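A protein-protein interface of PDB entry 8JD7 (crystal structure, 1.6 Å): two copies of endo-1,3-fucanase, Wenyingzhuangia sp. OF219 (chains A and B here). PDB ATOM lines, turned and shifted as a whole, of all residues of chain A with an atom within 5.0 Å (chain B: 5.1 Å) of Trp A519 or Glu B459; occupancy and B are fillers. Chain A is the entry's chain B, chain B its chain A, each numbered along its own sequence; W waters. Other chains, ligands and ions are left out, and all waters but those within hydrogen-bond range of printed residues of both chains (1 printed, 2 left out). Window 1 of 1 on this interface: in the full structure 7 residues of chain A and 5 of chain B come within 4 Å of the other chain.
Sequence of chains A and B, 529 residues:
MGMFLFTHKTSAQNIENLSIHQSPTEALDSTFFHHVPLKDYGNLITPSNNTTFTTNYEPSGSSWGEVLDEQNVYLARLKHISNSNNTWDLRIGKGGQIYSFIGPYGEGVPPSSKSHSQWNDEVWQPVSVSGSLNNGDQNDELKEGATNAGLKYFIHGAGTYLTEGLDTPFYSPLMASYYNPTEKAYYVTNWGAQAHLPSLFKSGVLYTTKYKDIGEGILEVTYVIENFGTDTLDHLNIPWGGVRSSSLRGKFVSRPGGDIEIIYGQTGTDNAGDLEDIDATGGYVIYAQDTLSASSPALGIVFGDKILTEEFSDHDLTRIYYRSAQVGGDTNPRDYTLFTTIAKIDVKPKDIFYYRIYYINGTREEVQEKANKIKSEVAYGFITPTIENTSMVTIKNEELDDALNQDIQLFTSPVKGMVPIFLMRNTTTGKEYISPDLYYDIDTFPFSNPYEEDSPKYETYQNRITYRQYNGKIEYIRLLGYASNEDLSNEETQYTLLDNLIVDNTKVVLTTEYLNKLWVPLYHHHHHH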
ATOM      1  N   ALA A 483      -4.334  13.943 -14.550  1.00  0.00           N
ATOM      2  CA  ALA A 483      -4.577  12.878 -13.584  1.00  0.00           C
ATOM      3  C   ALA A 483      -4.279  11.535 -14.227  1.00  0.00           C
ATOM      4  O   ALA A 483      -4.674  11.279 -15.368  1.00  0.00           O
ATOM      5  CB  ALA A 483      -6.024  12.891 -13.079  1.00  0.00           C
ATOM      6  N   SER A 484      -3.607  10.663 -13.479  1.00  0.00           N
ATOM      7  CA  SER A 484      -3.345   9.317 -13.974  1.00  0.00           C
ATOM      8  C   SER A 484      -4.640   8.563 -14.247  1.00  0.00           C
ATOM      9  O   SER A 484      -5.610   8.662 -13.489  1.00  0.00           O
ATOM     10  CB  SER A 484      -2.502   8.533 -12.973  1.00  0.00           C
ATOM     11  OG  SER A 484      -2.179   7.263 -13.511  1.00  0.00           O
ATOM     12  N   ASN A 485      -4.649   7.812 -15.348  1.00  0.00           N
ATOM     13  CA  ASN A 485      -5.738   6.902 -15.674  1.00  0.00           C
ATOM     14  C   ASN A 485      -5.576   5.543 -15.006  1.00  0.00           C
ATOM     15  O   ASN A 485      -6.365   4.629 -15.276  1.00  0.00           O
ATOM     16  CB  ASN A 485      -5.834   6.706 -17.190  1.00  0.00           C
ATOM     17  CG  ASN A 485      -4.556   6.140 -17.783  1.00  0.00           C
ATOM     18  OD1 ASN A 485      -3.458   6.606 -17.479  1.00  0.00           O
ATOM     19  ND2 ASN A 485      -4.693   5.131 -18.633  1.00  0.00           N
ATOM     20  N   GLU A 486      -4.562   5.378 -14.163  1.00  0.00           N
ATOM     21  CA  GLU A 486      -4.354   4.112 -13.485  1.00  0.00           C
ATOM     22  C   GLU A 486      -3.727   4.369 -12.123  1.00  0.00           C
ATOM     23  O   GLU A 486      -3.085   5.396 -11.886  1.00  0.00           O
ATOM     24  CB  GLU A 486      -3.506   3.159 -14.341  1.00  0.00           C
ATOM     25  CG  GLU A 486      -2.086   3.617 -14.606  1.00  0.00           C
ATOM     26  CD  GLU A 486      -1.447   2.854 -15.759  1.00  0.00           C
ATOM     27  OE1 GLU A 486      -2.188   2.211 -16.535  1.00  0.00           O
ATOM     28  OE2 GLU A 486      -0.205   2.896 -15.890  1.00  0.00           O
ATOM     29  N   ASP A 487      -3.962   3.423 -11.221  1.00  0.00           N
ATOM     30  CA  ASP A 487      -3.470   3.490  -9.851  1.00  0.00           C
ATOM     31  C   ASP A 487      -1.947   3.386  -9.836  1.00  0.00           C
ATOM     32  O   ASP A 487      -1.384   2.360 -10.238  1.00  0.00           O
ATOM     33  CB  ASP A 487      -4.116   2.361  -9.050  1.00  0.00           C
ATOM     34  CG  ASP A 487      -3.707   2.342  -7.589  1.00  0.00           C
ATOM     35  OD1 ASP A 487      -2.924   3.205  -7.146  1.00  0.00           O
ATOM     36  OD2 ASP A 487      -4.198   1.447  -6.867  1.00  0.00           O
ATOM     37  N   GLN A 494       0.352   6.293  -1.729  1.00  0.00           N
ATOM     38  CA  GLN A 494      -0.839   5.608  -2.201  1.00  0.00           C
ATOM     39  C   GLN A 494      -1.671   6.551  -3.061  1.00  0.00           C
ATOM     40  O   GLN A 494      -1.728   7.758  -2.812  1.00  0.00           O
ATOM     41  CB  GLN A 494      -1.675   5.104  -1.028  1.00  0.00           C
ATOM     42  CG  GLN A 494      -2.763   4.140  -1.436  1.00  0.00           C
ATOM     43  CD  GLN A 494      -3.434   3.486  -0.247  1.00  0.00           C
ATOM     44  OE1 GLN A 494      -2.800   3.238   0.781  1.00  0.00           O
ATOM     45  NE2 GLN A 494      -4.728   3.199  -0.378  1.00  0.00           N
ATOM     46  N   TYR A 495      -2.305   5.989  -4.086  1.00  0.00           N
ATOM     47  CA  TYR A 495      -3.188   6.728  -4.976  1.00  0.00           C
ATOM     48  C   TYR A 495      -4.638   6.340  -4.711  1.00  0.00           C
ATOM     49  O   TYR A 495      -4.938   5.208  -4.324  1.00  0.00           O
ATOM     50  CB  TYR A 495      -2.835   6.467  -6.448  1.00  0.00           C
ATOM     51  CG  TYR A 495      -1.739   7.365  -6.986  1.00  0.00           C
ATOM     52  CD1 TYR A 495      -0.457   7.335  -6.450  1.00  0.00           C
ATOM     53  CD2 TYR A 495      -1.983   8.221  -8.053  1.00  0.00           C
ATOM     54  CE1 TYR A 495       0.549   8.162  -6.945  1.00  0.00           C
ATOM     55  CE2 TYR A 495      -0.991   9.037  -8.555  1.00  0.00           C
ATOM     56  CZ  TYR A 495       0.273   9.008  -8.004  1.00  0.00           C
ATOM     57  OH  TYR A 495       1.258   9.833  -8.510  1.00  0.00           O
ATOM     58  N   THR A 496      -5.535   7.300  -4.910  1.00  0.00           N
ATOM     59  CA  THR A 496      -6.962   7.093  -4.738  1.00  0.00           C
ATOM     60  C   THR A 496      -7.702   7.695  -5.924  1.00  0.00           C
ATOM     61  O   THR A 496      -7.142   8.471  -6.701  1.00  0.00           O
ATOM     62  CB  THR A 496      -7.466   7.722  -3.433  1.00  0.00           C
ATOM     63  OG1 THR A 496      -8.820   7.319  -3.196  1.00  0.00           O
ATOM     64  CG2 THR A 496      -7.402   9.247  -3.517  1.00  0.00           C
ATOM     65  N   LEU A 497      -8.970   7.320  -6.062  1.00  0.00           N
ATOM     66  CA  LEU A 497      -9.815   7.923  -7.085  1.00  0.00           C
ATOM     67  C   LEU A 497     -10.155   9.356  -6.691  1.00  0.00           C
ATOM     68  O   LEU A 497     -10.510   9.628  -5.537  1.00  0.00           O
ATOM     69  CB  LEU A 497     -11.087   7.096  -7.264  1.00  0.00           C
ATOM     70  CG  LEU A 497     -10.966   5.868  -8.172  1.00  0.00           C
ATOM     71  CD1 LEU A 497     -12.322   5.219  -8.379  1.00  0.00           C
ATOM     72  CD2 LEU A 497     -10.345   6.236  -9.517  1.00  0.00           C
ATOM     73  N   LEU A 498     -10.018  10.285  -7.646  1.00  0.00           N
ATOM     74  CA  LEU A 498     -10.407  11.670  -7.397  1.00  0.00           C
ATOM     75  C   LEU A 498     -11.841  11.752  -6.887  1.00  0.00           C
ATOM     76  O   LEU A 498     -12.163  12.603  -6.052  1.00  0.00           O
ATOM     77  CB  LEU A 498     -10.250  12.498  -8.680  1.00  0.00           C
ATOM     78  CG  LEU A 498     -10.532  14.005  -8.591  1.00  0.00           C
ATOM     79  CD1 LEU A 498      -9.724  14.657  -7.479  1.00  0.00           C
ATOM     80  CD2 LEU A 498     -10.280  14.684  -9.939  1.00  0.00           C
ATOM     81  N   ASN A 500     -13.302  10.042  -4.746  1.00  0.00           N
ATOM     82  CA  ASN A 500     -13.382   9.862  -3.295  1.00  0.00           C
ATOM     83  C   ASN A 500     -13.078  11.130  -2.523  1.00  0.00           C
ATOM     84  O   ASN A 500     -13.330  11.178  -1.310  1.00  0.00           O
ATOM     85  CB  ASN A 500     -12.401   8.783  -2.835  1.00  0.00           C
ATOM     86  CG  ASN A 500     -12.760   7.416  -3.344  1.00  0.00           C
ATOM     87  OD1 ASN A 500     -13.931   7.109  -3.558  1.00  0.00           O
ATOM     88  ND2 ASN A 500     -11.748   6.575  -3.535  1.00  0.00           N
ATOM     89  N   LYS A 517     -12.351   6.907 -12.963  1.00  0.00           N
ATOM     90  CA  LYS A 517     -11.266   6.751 -13.917  1.00  0.00           C
ATOM     91  C   LYS A 517      -9.991   7.495 -13.551  1.00  0.00           C
ATOM     92  O   LYS A 517      -8.921   7.101 -14.026  1.00  0.00           O
ATOM     93  CB  LYS A 517     -11.704   7.210 -15.321  1.00  0.00           C
ATOM     94  CG  LYS A 517     -12.919   6.481 -15.894  1.00  0.00           C
ATOM     95  CD  LYS A 517     -12.695   6.143 -17.365  1.00  0.00           C
ATOM     96  CE  LYS A 517     -13.960   5.637 -18.054  1.00  0.00           C
ATOM     97  NZ  LYS A 517     -14.290   6.481 -19.237  1.00  0.00           N
ATOM     98  N   LEU A 518     -10.061   8.543 -12.734  1.00  0.00           N
ATOM     99  CA  LEU A 518      -8.933   9.440 -12.510  1.00  0.00           C
ATOM    100  C   LEU A 518      -8.341   9.197 -11.130  1.00  0.00           C
ATOM    101  O   LEU A 518      -9.070   9.183 -10.132  1.00  0.00           O
ATOM    102  CB  LEU A 518      -9.357  10.904 -12.648  1.00  0.00           C
ATOM    103  CG  LEU A 518      -9.535  11.488 -14.053  1.00  0.00           C
ATOM    104  CD1 LEU A 518     -10.559  10.738 -14.878  1.00  0.00           C
ATOM    105  CD2 LEU A 518      -9.941  12.939 -13.936  1.00  0.00           C
ATOM    106  N   TRP A 519      -7.021   9.022 -11.075  1.00  0.00           N
ATOM    107  CA  TRP A 519      -6.310   8.713  -9.840  1.00  0.00           C
ATOM    108  C   TRP A 519      -5.334   9.829  -9.486  1.00  0.00           C
ATOM    109  O   TRP A 519      -4.632  10.347 -10.359  1.00  0.00           O
ATOM    110  CB  TRP A 519      -5.530   7.399  -9.965  1.00  0.00           C
ATOM    111  CG  TRP A 519      -6.384   6.197 -10.203  1.00  0.00           C
ATOM    112  CD1 TRP A 519      -7.018   5.853 -11.365  1.00  0.00           C
ATOM    113  CD2 TRP A 519      -6.715   5.184  -9.247  1.00  0.00           C
ATOM    114  NE1 TRP A 519      -7.714   4.676 -11.189  1.00  0.00           N
ATOM    115  CE2 TRP A 519      -7.546   4.250  -9.897  1.00  0.00           C
ATOM    116  CE3 TRP A 519      -6.382   4.975  -7.903  1.00  0.00           C
ATOM    117  CZ2 TRP A 519      -8.050   3.119  -9.247  1.00  0.00           C
ATOM    118  CZ3 TRP A 519      -6.887   3.856  -7.259  1.00  0.00           C
ATOM    119  CH2 TRP A 519      -7.711   2.943  -7.932  1.00  0.00           C
ATOM    120  N   VAL A 520      -5.288  10.182  -8.203  1.00  0.00           N
ATOM    121  CA  VAL A 520      -4.323  11.143  -7.664  1.00  0.00           C
ATOM    122  C   VAL A 520      -3.786  10.617  -6.341  1.00  0.00           C
ATOM    123  O   VAL A 520      -4.388   9.732  -5.718  1.00  0.00           O
ATOM    124  CB  VAL A 520      -4.952  12.536  -7.459  1.00  0.00           C
ATOM    125  CG1 VAL A 520      -5.424  13.106  -8.788  1.00  0.00           C
ATOM    126  CG2 VAL A 520      -6.094  12.465  -6.465  1.00  0.00           C
ATOM    127  N   PRO A 521      -2.645  11.145  -5.883  1.00  0.00           N
ATOM    128  CA  PRO A 521      -2.114  10.727  -4.578  1.00  0.00           C
ATOM    129  C   PRO A 521      -3.103  10.967  -3.447  1.00  0.00           C
ATOM    130  O   PRO A 521      -3.791  11.990  -3.394  1.00  0.00           O
ATOM    131  CB  PRO A 521      -0.857  11.591  -4.418  1.00  0.00           C
ATOM    132  CG  PRO A 521      -0.396  11.762  -5.825  1.00  0.00           C
ATOM    133  CD  PRO A 521      -1.676  11.999  -6.597  1.00  0.00           C
ATOM    134  N   LEU A 522      -3.175   9.993  -2.547  1.00  0.00           N
ATOM    135  CA  LEU A 522      -4.015  10.075  -1.360  1.00  0.00           C
ATOM    136  C   LEU A 522      -3.235  10.711  -0.219  1.00  0.00           C
ATOM    137  O   LEU A 522      -2.101  10.311   0.066  1.00  0.00           O
ATOM    138  CB  LEU A 522      -4.501   8.685  -0.945  1.00  0.00           C
ATOM    139  CG  LEU A 522      -5.403   8.620   0.294  1.00  0.00           C
ATOM    140  CD1 LEU A 522      -6.714   9.362   0.089  1.00  0.00           C
ATOM    141  CD2 LEU A 522      -5.655   7.174   0.704  1.00  0.00           C
ATOM    142  N   GLU B 453     -11.422  -0.471   4.651  1.00  0.00           N
ATOM    143  CA  GLU B 453     -11.056   0.838   4.116  1.00  0.00           C
ATOM    144  C   GLU B 453      -9.565   1.118   4.283  1.00  0.00           C
ATOM    145  O   GLU B 453      -8.950   1.748   3.416  1.00  0.00           O
ATOM    146  CB  GLU B 453     -11.890   1.926   4.790  1.00  0.00           C
ATOM    147  N   SER B 455      -7.177  -0.929   3.977  1.00  0.00           N
ATOM    148  CA  SER B 455      -6.289  -1.767   3.182  1.00  0.00           C
ATOM    149  C   SER B 455      -5.712  -0.975   2.007  1.00  0.00           C
ATOM    150  O   SER B 455      -6.405  -0.141   1.419  1.00  0.00           O
ATOM    151  CB  SER B 455      -7.026  -2.997   2.658  1.00  0.00           C
ATOM    152  OG  SER B 455      -6.191  -3.738   1.784  1.00  0.00           O
ATOM    153  N   PRO B 456      -4.445  -1.208   1.661  1.00  0.00           N
ATOM    154  CA  PRO B 456      -3.889  -0.569   0.459  1.00  0.00           C
ATOM    155  C   PRO B 456      -4.665  -0.912  -0.796  1.00  0.00           C
ATOM    156  O   PRO B 456      -4.736  -0.100  -1.726  1.00  0.00           O
ATOM    157  CB  PRO B 456      -2.459  -1.123   0.396  1.00  0.00           C
ATOM    158  CG  PRO B 456      -2.134  -1.531   1.793  1.00  0.00           C
ATOM    159  CD  PRO B 456      -3.426  -1.924   2.450  1.00  0.00           C
ATOM    160  N   LYS B 457      -5.260  -2.100  -0.836  1.00  0.00           N
ATOM    161  CA  LYS B 457      -5.984  -2.599  -1.995  1.00  0.00           C
ATOM    162  C   LYS B 457      -7.420  -2.097  -2.053  1.00  0.00           C
ATOM    163  O   LYS B 457      -8.123  -2.381  -3.028  1.00  0.00           O
ATOM    164  CB  LYS B 457      -5.962  -4.129  -1.973  1.00  0.00           C
ATOM    165  CG  LYS B 457      -4.552  -4.712  -1.996  1.00  0.00           C
ATOM    166  CD  LYS B 457      -4.517  -6.166  -2.449  1.00  0.00           C
ATOM    167  CE  LYS B 457      -3.082  -6.674  -2.522  1.00  0.00           C
ATOM    168  NZ  LYS B 457      -2.970  -8.108  -2.907  1.00  0.00           N
ATOM    169  N   TYR B 458      -7.868  -1.344  -1.046  1.00  0.00           N
ATOM    170  CA  TYR B 458      -9.279  -0.976  -0.959  1.00  0.00           C
ATOM    171  C   TYR B 458      -9.742  -0.198  -2.189  1.00  0.00           C
ATOM    172  O   TYR B 458     -10.808  -0.486  -2.746  1.00  0.00           O
ATOM    173  CB  TYR B 458      -9.525  -0.172   0.318  1.00  0.00           C
ATOM    174  CG  TYR B 458     -10.924   0.388   0.425  1.00  0.00           C
ATOM    175  CD1 TYR B 458     -11.968  -0.397   0.890  1.00  0.00           C
ATOM    176  CD2 TYR B 458     -11.203   1.695   0.049  1.00  0.00           C
ATOM    177  CE1 TYR B 458     -13.249   0.105   0.990  1.00  0.00           C
ATOM    178  CE2 TYR B 458     -12.481   2.206   0.150  1.00  0.00           C
ATOM    179  CZ  TYR B 458     -13.500   1.405   0.619  1.00  0.00           C
ATOM    180  OH  TYR B 458     -14.776   1.907   0.718  1.00  0.00           O
ATOM    181  N   GLU B 459      -8.955   0.793  -2.630  1.00  0.00           N
ATOM    182  CA  GLU B 459      -9.406   1.659  -3.717  1.00  0.00           C
ATOM    183  C   GLU B 459      -9.494   0.916  -5.039  1.00  0.00           C
ATOM    184  O   GLU B 459     -10.266   1.316  -5.920  1.00  0.00           O
ATOM    185  CB  GLU B 459      -8.481   2.865  -3.873  1.00  0.00           C
ATOM    186  CG  GLU B 459      -8.658   3.949  -2.824  1.00  0.00           C
ATOM    187  CD  GLU B 459      -8.008   3.589  -1.514  1.00  0.00           C
ATOM    188  OE1 GLU B 459      -6.930   2.958  -1.545  1.00  0.00           O
ATOM    189  OE2 GLU B 459      -8.574   3.940  -0.457  1.00  0.00           O
ATOM    190  N   THR B 460      -8.702  -0.148  -5.203  1.00  0.00           N
ATOM    191  CA  THR B 460      -8.747  -0.933  -6.431  1.00  0.00           C
ATOM    192  C   THR B 460     -10.143  -1.481  -6.699  1.00  0.00           C
ATOM    193  O   THR B 460     -10.561  -1.578  -7.860  1.00  0.00           O
ATOM    194  CB  THR B 460      -7.729  -2.079  -6.350  1.00  0.00           C
ATOM    195  OG1 THR B 460      -6.403  -1.555  -6.180  1.00  0.00           O
ATOM    196  CG2 THR B 460      -7.774  -2.932  -7.596  1.00  0.00           C
ATOM    197  N   TYR B 461     -10.891  -1.810  -5.646  1.00  0.00           N
ATOM    198  CA  TYR B 461     -12.131  -2.561  -5.786  1.00  0.00           C
ATOM    199  C   TYR B 461     -13.374  -1.735  -5.474  1.00  0.00           C
ATOM    200  O   TYR B 461     -14.462  -2.298  -5.326  1.00  0.00           O
ATOM    201  CB  TYR B 461     -12.049  -3.815  -4.919  1.00  0.00           C
ATOM    202  CG  TYR B 461     -10.914  -4.678  -5.401  1.00  0.00           C
ATOM    203  CD1 TYR B 461     -11.012  -5.372  -6.606  1.00  0.00           C
ATOM    204  CD2 TYR B 461      -9.714  -4.729  -4.714  1.00  0.00           C
ATOM    205  CE1 TYR B 461      -9.956  -6.134  -7.080  1.00  0.00           C
ATOM    206  CE2 TYR B 461      -8.664  -5.502  -5.167  1.00  0.00           C
ATOM    207  CZ  TYR B 461      -8.789  -6.200  -6.352  1.00  0.00           C
ATOM    208  OH  TYR B 461      -7.723  -6.945  -6.792  1.00  0.00           O
ATOM    209  N   GLN B 462     -13.242  -0.408  -5.422  1.00  0.00           N
ATOM    210  CA  GLN B 462     -14.395   0.478  -5.358  1.00  0.00           C
ATOM    211  C   GLN B 462     -15.011   0.646  -6.742  1.00  0.00           C
ATOM    212  O   GLN B 462     -14.295   0.754  -7.741  1.00  0.00           O
ATOM    213  CB  GLN B 462     -13.991   1.854  -4.821  1.00  0.00           C
ATOM    214  CG  GLN B 462     -13.394   1.870  -3.430  1.00  0.00           C
ATOM    215  CD  GLN B 462     -13.161   3.287  -2.937  1.00  0.00           C
ATOM    216  OE1 GLN B 462     -12.189   3.941  -3.326  1.00  0.00           O
ATOM    217  NE2 GLN B 462     -14.066   3.779  -2.094  1.00  0.00           N
HETATM  218  O   HOH W   1      -5.353  -0.694  -8.333  1.00  0.00           O
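Among the printed residues, merely in contact across the chains: Thr A496 with Glu B459, Gln A494 with Pro B456, Trp A519 with Glu B459 and Asp A487 with Thr B460.
No position is printed for both chains.
Water W1 lies within hydrogen-bond range of OG1 of Thr B460 (2.5 Å) and OD2 of Asp A487 (2.8 Å).
OH of Tyr B458 sits close to NE2 of Gln B462 (3.5 Å). The backbone carbonyl oxygen of Gln A494 sits at hydrogen-bond distance from the backbone NH of Leu A522 (2.7 Å). O of Val A520 sits at hydrogen-bond distance from N of Thr A496. ND2 of Asn A500 sits at hydrogen-bond distance from OG1 of Thr A496 (3.0 Å). The backbone carbonyl oxygen (O) of Ser A484 is in hydrogen-bond range of the backbone NH (N) of Trp A519, 2.8 Å away.
Of the 17 printed residues of chain A, 5 touch a printed residue of chain B. Hydrophobic or aromatic side chains of chain A that line the printed part of chain B: Trp A519. Of the 9 printed residues of chain B, 4 touch a printed residue of chain A. Along chain B the printed residues that touch a printed residue of chain A span positions 456 to 462.
The side-chain amide oxygen of Gln B462 lies within hydrogen-bond range of the side-chain amide nitrogen of Asn A500, at 2.7 Å. The side-chain carboxylate (OE1) of Glu B459 is in hydrogen-bond range of the side-chain amide nitrogen (NE2) of Gln A494 (2.5 Å).
Of chain B, only Glu B459 comes within 4 Å of Trp A519. Glu B459 touches three residues of chain A. Printed residues of chain A within 4 Å of Pro B456: Gln A494 (3.6 Å). Printed residues of chain B within 4 Å of Asp A487: Thr B460. The nearest printed residue of chain A that does not touch Glu B459 is Tyr A495 (4.1 Å). The nearest printed residue of chain A that does not touch Thr B460 is Trp A519 (4.2 Å).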
